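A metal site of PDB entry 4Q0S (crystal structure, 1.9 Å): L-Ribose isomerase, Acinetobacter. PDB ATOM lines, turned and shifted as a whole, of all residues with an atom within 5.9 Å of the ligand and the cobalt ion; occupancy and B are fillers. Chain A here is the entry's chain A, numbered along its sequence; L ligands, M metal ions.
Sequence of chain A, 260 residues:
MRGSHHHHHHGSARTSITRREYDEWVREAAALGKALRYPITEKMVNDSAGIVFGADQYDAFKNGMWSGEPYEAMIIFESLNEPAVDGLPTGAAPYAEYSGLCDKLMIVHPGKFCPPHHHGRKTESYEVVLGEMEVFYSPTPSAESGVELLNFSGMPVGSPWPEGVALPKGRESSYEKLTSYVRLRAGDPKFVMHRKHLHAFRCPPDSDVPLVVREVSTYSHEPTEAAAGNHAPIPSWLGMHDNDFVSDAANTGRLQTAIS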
ATOM      1  N   ILE A  51      -0.266 -19.006  33.293  1.00  0.00           N
ATOM      2  CA  ILE A  51       0.754 -19.787  32.611  1.00  0.00           C
ATOM      3  C   ILE A  51       1.751 -18.972  31.777  1.00  0.00           C
ATOM      4  O   ILE A  51       1.374 -18.077  31.024  1.00  0.00           O
ATOM      5  CB  ILE A  51       0.082 -20.822  31.683  1.00  0.00           C
ATOM      6  CG1 ILE A  51      -0.913 -21.661  32.488  1.00  0.00           C
ATOM      7  CG2 ILE A  51       1.129 -21.732  31.032  1.00  0.00           C
ATOM      8  CD1 ILE A  51      -1.892 -22.452  31.618  1.00  0.00           C
ATOM      9  N   PHE A  53       4.781 -19.799  29.114  1.00  0.00           N
ATOM     10  CA  PHE A  53       5.362 -20.883  28.322  1.00  0.00           C
ATOM     11  C   PHE A  53       6.864 -20.825  28.078  1.00  0.00           C
ATOM     12  O   PHE A  53       7.313 -20.564  26.954  1.00  0.00           O
ATOM     13  CB  PHE A  53       4.632 -21.003  26.988  1.00  0.00           C
ATOM     14  CG  PHE A  53       3.151 -21.271  27.118  1.00  0.00           C
ATOM     15  CD1 PHE A  53       2.240 -20.218  27.212  1.00  0.00           C
ATOM     16  CD2 PHE A  53       2.666 -22.579  27.146  1.00  0.00           C
ATOM     17  CE1 PHE A  53       0.877 -20.462  27.324  1.00  0.00           C
ATOM     18  CE2 PHE A  53       1.303 -22.835  27.264  1.00  0.00           C
ATOM     19  CZ  PHE A  53       0.404 -21.777  27.352  1.00  0.00           C
ATOM     20  N   MET A  74      -0.642 -16.971  29.247  1.00  0.00           N
ATOM     21  CA  MET A  74      -2.089 -16.848  29.292  1.00  0.00           C
ATOM     22  C   MET A  74      -2.603 -17.347  30.616  1.00  0.00           C
ATOM     23  O   MET A  74      -1.861 -17.914  31.427  1.00  0.00           O
ATOM     24  CB  MET A  74      -2.715 -17.701  28.195  1.00  0.00           C
ATOM     25  CG  MET A  74      -2.602 -19.198  28.517  1.00  0.00           C
ATOM     26  SD  MET A  74      -3.008 -20.263  27.136  1.00  0.00           S
ATOM     27  CE  MET A  74      -4.770 -19.882  26.963  1.00  0.00           C
ATOM     28  N   ILE A  76      -5.811 -19.628  32.443  1.00  0.00           N
ATOM     29  CA  ILE A  76      -6.859 -20.598  32.176  1.00  0.00           C
ATOM     30  C   ILE A  76      -7.538 -20.937  33.490  1.00  0.00           C
ATOM     31  O   ILE A  76      -6.869 -21.306  34.453  1.00  0.00           O
ATOM     32  CB  ILE A  76      -6.317 -21.908  31.562  1.00  0.00           C
ATOM     33  CG1 ILE A  76      -5.649 -21.629  30.217  1.00  0.00           C
ATOM     34  CG2 ILE A  76      -7.450 -22.915  31.393  1.00  0.00           C
ATOM     35  CD1 ILE A  76      -5.034 -22.866  29.557  1.00  0.00           C
ATOM     36  N   LYS A 104     -13.307 -24.503  30.149  1.00  0.00           N
ATOM     37  CA  LYS A 104     -12.417 -23.536  30.774  1.00  0.00           C
ATOM     38  C   LYS A 104     -12.569 -22.172  30.133  1.00  0.00           C
ATOM     39  O   LYS A 104     -13.089 -22.038  29.035  1.00  0.00           O
ATOM     40  CB  LYS A 104     -10.955 -23.985  30.642  1.00  0.00           C
ATOM     41  CG  LYS A 104     -10.393 -23.826  29.235  1.00  0.00           C
ATOM     42  CD  LYS A 104      -9.893 -25.158  28.668  1.00  0.00           C
ATOM     43  CE  LYS A 104     -11.031 -26.149  28.471  1.00  0.00           C
ATOM     44  NZ  LYS A 104     -10.603 -27.404  27.772  1.00  0.00           N
ATOM     45  N   MET A 106     -10.342 -18.874  29.027  1.00  0.00           N
ATOM     46  CA  MET A 106      -8.965 -18.511  28.752  1.00  0.00           C
ATOM     47  C   MET A 106      -8.868 -17.007  28.545  1.00  0.00           C
ATOM     48  O   MET A 106      -9.668 -16.406  27.838  1.00  0.00           O
ATOM     49  CB  MET A 106      -8.455 -19.259  27.512  1.00  0.00           C
ATOM     50  CG  MET A 106      -8.624 -20.762  27.638  1.00  0.00           C
ATOM     51  SD  MET A 106      -7.886 -21.709  26.292  1.00  0.00           S
ATOM     52  CE  MET A 106      -8.943 -21.287  24.955  1.00  0.00           C
ATOM     53  N   CYS A 114      -1.121 -18.101  22.916  1.00  0.00           N
ATOM     54  CA  CYS A 114      -1.221 -19.445  23.462  1.00  0.00           C
ATOM     55  C   CYS A 114      -0.353 -20.017  22.327  1.00  0.00           C
ATOM     56  O   CYS A 114      -0.763 -20.029  21.166  1.00  0.00           O
ATOM     57  CB  CYS A 114      -2.630 -20.011  23.365  1.00  0.00           C
ATOM     58  SG  CYS A 114      -2.711 -21.796  23.778  1.00  0.00           S
ATOM     59  N   HIS A 117       0.983 -25.613  19.170  1.00  0.00           N
ATOM     60  CA  HIS A 117       0.988 -26.949  19.753  1.00  0.00           C
ATOM     61  C   HIS A 117      -0.153 -27.742  19.145  1.00  0.00           C
ATOM     62  O   HIS A 117      -0.976 -27.193  18.406  1.00  0.00           O
ATOM     63  CB  HIS A 117       0.803 -26.877  21.277  1.00  0.00           C
ATOM     64  CG  HIS A 117      -0.553 -26.376  21.698  1.00  0.00           C
ATOM     65  ND1 HIS A 117      -0.942 -25.068  21.542  1.00  0.00           N
ATOM     66  CD2 HIS A 117      -1.614 -27.033  22.212  1.00  0.00           C
ATOM     67  CE1 HIS A 117      -2.191 -24.928  21.949  1.00  0.00           C
ATOM     68  NE2 HIS A 117      -2.623 -26.105  22.362  1.00  0.00           N
ATOM     69  N   HIS A 119      -2.690 -31.550  19.913  1.00  0.00           N
ATOM     70  CA  HIS A 119      -3.061 -32.614  20.837  1.00  0.00           C
ATOM     71  C   HIS A 119      -3.319 -33.912  20.083  1.00  0.00           C
ATOM     72  O   HIS A 119      -3.919 -33.902  19.014  1.00  0.00           O
ATOM     73  CB  HIS A 119      -4.336 -32.218  21.597  1.00  0.00           C
ATOM     74  CG  HIS A 119      -4.248 -30.864  22.242  1.00  0.00           C
ATOM     75  ND1 HIS A 119      -3.462 -30.618  23.338  1.00  0.00           N
ATOM     76  CD2 HIS A 119      -4.826 -29.692  21.914  1.00  0.00           C
ATOM     77  CE1 HIS A 119      -3.552 -29.338  23.662  1.00  0.00           C
ATOM     78  NE2 HIS A 119      -4.372 -28.752  22.816  1.00  0.00           N
ATOM     79  N   LYS A 122      -7.079 -34.579  22.359  1.00  0.00           N
ATOM     80  CA  LYS A 122      -8.050 -33.508  22.574  1.00  0.00           C
ATOM     81  C   LYS A 122      -8.499 -32.644  21.397  1.00  0.00           C
ATOM     82  O   LYS A 122      -7.684 -32.030  20.705  1.00  0.00           O
ATOM     83  CB  LYS A 122      -7.572 -32.571  23.684  1.00  0.00           C
ATOM     84  CG  LYS A 122      -8.576 -31.452  24.013  1.00  0.00           C
ATOM     85  CD  LYS A 122      -8.133 -30.605  25.195  1.00  0.00           C
ATOM     86  CE  LYS A 122      -6.880 -29.807  24.876  1.00  0.00           C
ATOM     87  NZ  LYS A 122      -6.388 -29.067  26.069  1.00  0.00           N
ATOM     88  N   GLU A 124     -10.824 -29.400  20.449  1.00  0.00           N
ATOM     89  CA  GLU A 124     -11.314 -28.178  21.091  1.00  0.00           C
ATOM     90  C   GLU A 124     -12.357 -27.440  20.252  1.00  0.00           C
ATOM     91  O   GLU A 124     -12.508 -27.693  19.054  1.00  0.00           O
ATOM     92  CB  GLU A 124     -10.155 -27.219  21.347  1.00  0.00           C
ATOM     93  CG  GLU A 124      -8.968 -27.813  22.104  1.00  0.00           C
ATOM     94  CD  GLU A 124      -7.725 -26.909  22.073  1.00  0.00           C
ATOM     95  OE1 GLU A 124      -7.779 -25.795  21.517  1.00  0.00           O
ATOM     96  OE2 GLU A 124      -6.679 -27.328  22.615  1.00  0.00           O
ATOM     97  N   TYR A 126     -14.008 -23.210  20.218  1.00  0.00           N
ATOM     98  CA  TYR A 126     -13.852 -21.885  20.795  1.00  0.00           C
ATOM     99  C   TYR A 126     -15.078 -21.009  20.707  1.00  0.00           C
ATOM    100  O   TYR A 126     -15.792 -21.005  19.706  1.00  0.00           O
ATOM    101  CB  TYR A 126     -12.700 -21.134  20.127  1.00  0.00           C
ATOM    102  CG  TYR A 126     -11.425 -21.921  19.954  1.00  0.00           C
ATOM    103  CD1 TYR A 126     -10.843 -22.566  21.036  1.00  0.00           C
ATOM    104  CD2 TYR A 126     -10.809 -22.010  18.707  1.00  0.00           C
ATOM    105  CE1 TYR A 126      -9.663 -23.290  20.892  1.00  0.00           C
ATOM    106  CE2 TYR A 126      -9.634 -22.730  18.542  1.00  0.00           C
ATOM    107  CZ  TYR A 126      -9.066 -23.371  19.633  1.00  0.00           C
ATOM    108  OH  TYR A 126      -7.912 -24.109  19.478  1.00  0.00           O
ATOM    109  N   HIS A 199      -2.095 -25.638  16.344  1.00  0.00           N
ATOM    110  CA  HIS A 199      -2.834 -24.401  16.525  1.00  0.00           C
ATOM    111  C   HIS A 199      -2.201 -23.499  17.564  1.00  0.00           C
ATOM    112  O   HIS A 199      -1.433 -23.943  18.420  1.00  0.00           O
ATOM    113  CB  HIS A 199      -4.304 -24.680  16.879  1.00  0.00           C
ATOM    114  CG  HIS A 199      -4.487 -25.495  18.117  1.00  0.00           C
ATOM    115  ND1 HIS A 199      -4.238 -26.857  18.170  1.00  0.00           N
ATOM    116  CD2 HIS A 199      -4.871 -25.143  19.371  1.00  0.00           C
ATOM    117  CE1 HIS A 199      -4.464 -27.304  19.383  1.00  0.00           C
ATOM    118  NE2 HIS A 199      -4.851 -26.286  20.136  1.00  0.00           N
ATOM    119  N   PHE A 201      -3.022 -19.099  19.106  1.00  0.00           N
ATOM    120  CA  PHE A 201      -3.903 -17.956  18.999  1.00  0.00           C
ATOM    121  C   PHE A 201      -3.416 -16.807  19.867  1.00  0.00           C
ATOM    122  O   PHE A 201      -2.696 -17.015  20.839  1.00  0.00           O
ATOM    123  CB  PHE A 201      -5.337 -18.352  19.347  1.00  0.00           C
ATOM    124  CG  PHE A 201      -5.511 -18.945  20.731  1.00  0.00           C
ATOM    125  CD1 PHE A 201      -5.615 -18.133  21.850  1.00  0.00           C
ATOM    126  CD2 PHE A 201      -5.597 -20.328  20.893  1.00  0.00           C
ATOM    127  CE1 PHE A 201      -5.817 -18.685  23.122  1.00  0.00           C
ATOM    128  CE2 PHE A 201      -5.796 -20.889  22.163  1.00  0.00           C
ATOM    129  CZ  PHE A 201      -5.910 -20.067  23.272  1.00  0.00           C
ATOM    130  N   GLU A 215     -13.533 -22.288  26.268  1.00  0.00           N
ATOM    131  CA  GLU A 215     -13.173 -23.495  25.515  1.00  0.00           C
ATOM    132  C   GLU A 215     -13.948 -24.692  26.025  1.00  0.00           C
ATOM    133  O   GLU A 215     -14.018 -24.946  27.228  1.00  0.00           O
ATOM    134  CB  GLU A 215     -11.670 -23.800  25.620  1.00  0.00           C
ATOM    135  CG  GLU A 215     -11.301 -25.109  24.902  1.00  0.00           C
ATOM    136  CD  GLU A 215      -9.841 -25.467  25.044  1.00  0.00           C
ATOM    137  OE1 GLU A 215      -8.996 -24.717  24.519  1.00  0.00           O
ATOM    138  OE2 GLU A 215      -9.536 -26.510  25.670  1.00  0.00           O
ATOM    139  N   SER A 220      -8.873 -33.055  29.239  1.00  0.00           N
ATOM    140  CA  SER A 220      -7.539 -32.471  29.183  1.00  0.00           C
ATOM    141  C   SER A 220      -6.553 -33.300  30.024  1.00  0.00           C
ATOM    142  O   SER A 220      -6.598 -33.287  31.251  1.00  0.00           O
ATOM    143  CB  SER A 220      -7.585 -31.032  29.685  1.00  0.00           C
ATOM    144  OG  SER A 220      -6.336 -30.391  29.520  1.00  0.00           O
ATOM    145  N   GLU A 222      -3.301 -33.488  31.494  1.00  0.00           N
ATOM    146  CA  GLU A 222      -2.170 -32.632  31.841  1.00  0.00           C
ATOM    147  C   GLU A 222      -1.710 -32.816  33.286  1.00  0.00           C
ATOM    148  O   GLU A 222      -2.353 -32.324  34.212  1.00  0.00           O
ATOM    149  CB  GLU A 222      -2.530 -31.163  31.624  1.00  0.00           C
ATOM    150  CG  GLU A 222      -2.904 -30.803  30.201  1.00  0.00           C
ATOM    151  CD  GLU A 222      -3.327 -29.348  30.062  1.00  0.00           C
ATOM    152  OE1 GLU A 222      -4.263 -28.935  30.777  1.00  0.00           O
ATOM    153  OE2 GLU A 222      -2.716 -28.628  29.237  1.00  0.00           O
ATOM    154  N   ASN A 243      -0.081 -32.805  25.408  1.00  0.00           N
ATOM    155  CA  ASN A 243       0.310 -31.488  24.900  1.00  0.00           C
ATOM    156  C   ASN A 243       1.627 -31.643  24.160  1.00  0.00           C
ATOM    157  O   ASN A 243       2.591 -32.180  24.700  1.00  0.00           O
ATOM    158  CB  ASN A 243       0.501 -30.473  26.032  1.00  0.00           C
ATOM    159  CG  ASN A 243      -0.807 -30.068  26.680  1.00  0.00           C
ATOM    160  OD1 ASN A 243      -1.872 -30.147  26.064  1.00  0.00           O
ATOM    161  ND2 ASN A 243      -0.730 -29.612  27.923  1.00  0.00           N
ATOM    162  N   PHE A 245       3.949 -29.087  22.245  1.00  0.00           N
ATOM    163  CA  PHE A 245       4.291 -27.752  21.784  1.00  0.00           C
ATOM    164  C   PHE A 245       5.400 -27.817  20.756  1.00  0.00           C
ATOM    165  O   PHE A 245       6.326 -28.623  20.882  1.00  0.00           O
ATOM    166  CB  PHE A 245       4.717 -26.892  22.977  1.00  0.00           C
ATOM    167  CG  PHE A 245       3.595 -26.587  23.927  1.00  0.00           C
ATOM    168  CD1 PHE A 245       2.808 -25.445  23.756  1.00  0.00           C
ATOM    169  CD2 PHE A 245       3.271 -27.464  24.963  1.00  0.00           C
ATOM    170  CE1 PHE A 245       1.721 -25.198  24.588  1.00  0.00           C
ATOM    171  CE2 PHE A 245       2.184 -27.229  25.802  1.00  0.00           C
ATOM    172  CZ  PHE A 245       1.404 -26.091  25.610  1.00  0.00           C
ATOM    173  N   ARG A 254       5.132 -24.982  30.855  1.00  0.00           N
ATOM    174  CA  ARG A 254       3.684 -25.116  30.820  1.00  0.00           C
ATOM    175  C   ARG A 254       3.129 -25.694  32.120  1.00  0.00           C
ATOM    176  O   ARG A 254       2.155 -25.178  32.677  1.00  0.00           O
ATOM    177  CB  ARG A 254       3.284 -26.013  29.633  1.00  0.00           C
ATOM    178  CG  ARG A 254       1.856 -25.824  29.134  1.00  0.00           C
ATOM    179  CD  ARG A 254       0.807 -26.126  30.202  1.00  0.00           C
ATOM    180  NE  ARG A 254      -0.549 -25.970  29.699  1.00  0.00           N
ATOM    181  CZ  ARG A 254      -1.645 -26.085  30.438  1.00  0.00           C
ATOM    182  NH1 ARG A 254      -2.839 -25.927  29.887  1.00  0.00           N
ATOM    183  NH2 ARG A 254      -1.548 -26.361  31.737  1.00  0.00           N
HETATM  184  C1  LIG L   1      -3.156 -24.630  26.345  1.00  0.00           C
HETATM  185  O1  LIG L   1      -2.047 -24.733  27.225  1.00  0.00           O
HETATM  186  C2  LIG L   1      -4.332 -25.398  26.926  1.00  0.00           C
HETATM  187  O2  LIG L   1      -4.101 -26.798  26.813  1.00  0.00           O
HETATM  188  C3  LIG L   1      -5.642 -24.996  26.210  1.00  0.00           C
HETATM  189  O3  LIG L   1      -6.758 -25.542  26.907  1.00  0.00           O
HETATM  190  C4  LIG L   1      -5.690 -25.432  24.744  1.00  0.00           C
HETATM  191  O4  LIG L   1      -4.761 -26.491  24.523  1.00  0.00           O
HETATM  192  C5  LIG L   1      -5.356 -24.254  23.836  1.00  0.00           C
HETATM  193  O5  LIG L   1      -5.563 -24.620  22.473  1.00  0.00           O
HETATM  194 CO    CO M   1      -4.860 -26.687  22.423  1.00  0.00          CO
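The cobalt ion is bound by the side-chain carboxylate (OE2) of Glu 124 (1.9 Å). O4 of the ligand binds the cobalt ion, at 2.1 Å. The cobalt ion is bound by NE2 of His 119, at 2.2 Å. The cobalt ion is bound by O5 of the ligand (2.2 Å). NE2 of His 117 binds the cobalt ion (2.3 Å). The cobalt ion is bound by NE2 of His 199, at 2.3 Å.
An oxygen (O1) of the ligand is in hydrogen-bond range of the guanidinium group (NH1) of Arg 254, 3.0 Å away. O3 of the ligand is in hydrogen-bond range of OE2 of Glu 215 (3.2 Å). The side-chain amino group (NZ) of Lys 122 is in hydrogen-bond range of an oxygen (O2) of the ligand (3.3 Å). O2 of the ligand lies within hydrogen-bond range of OE2 of Glu 222, at 3.3 Å.
Phe 53 touches the ligand (CZ to O1, 3.8 Å). Ile 76 touches the ligand (CD1 to C2, 3.7 Å). Lys 104 touches the ligand. Met 106 touches the ligand. Cys 114 touches the ligand (SG to C5, 3.6 Å). OH of Tyr 126 touches O5 of the ligand, at 3.8 Å. CE2 of Phe 201 touches O5 of the ligand, 3.8 Å away. Of the 20 residues printed, 15 come within 4 Å of the ligand. Along chain A the residues within 4 Å of the ligand span positions 53 to 254. The nearest printed residue that does not touch the ligand is Phe 245 (4.04 Å).
The side-chain amino group (NZ) of Lys 122 lies close to the side-chain carboxylate (OE2) of Glu 124, 3.9 Å away. OE1 of Glu 124 lies within hydrogen-bond range of OH of Tyr 126. The guanidinium group (NH1) of Arg 254 is in salt-bridge range of the side-chain carboxylate (OE2) of Glu 222, 2.8 Å away. The side-chain carboxylate of Glu 215 lies within salt-bridge range of the side-chain amino group of Lys 104, 2.5 Å away. The side-chain carboxylate of Glu 222 lies within hydrogen-bond range of the side-chain amide nitrogen of Asn 243, at 2.6 Å. The side-chain carboxylate of Glu 222 sits at hydrogen-bond distance from the side-chain hydroxyl of Ser 220 (2.8 Å). N of Cys 114 sits at hydrogen-bond distance from O of Phe 201 (2.8 Å). SG of Cys 114 sits at hydrogen-bond distance from SD of Met 74.
Of the 20 residues printed, 4 come within 4 Å of the cobalt ion.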
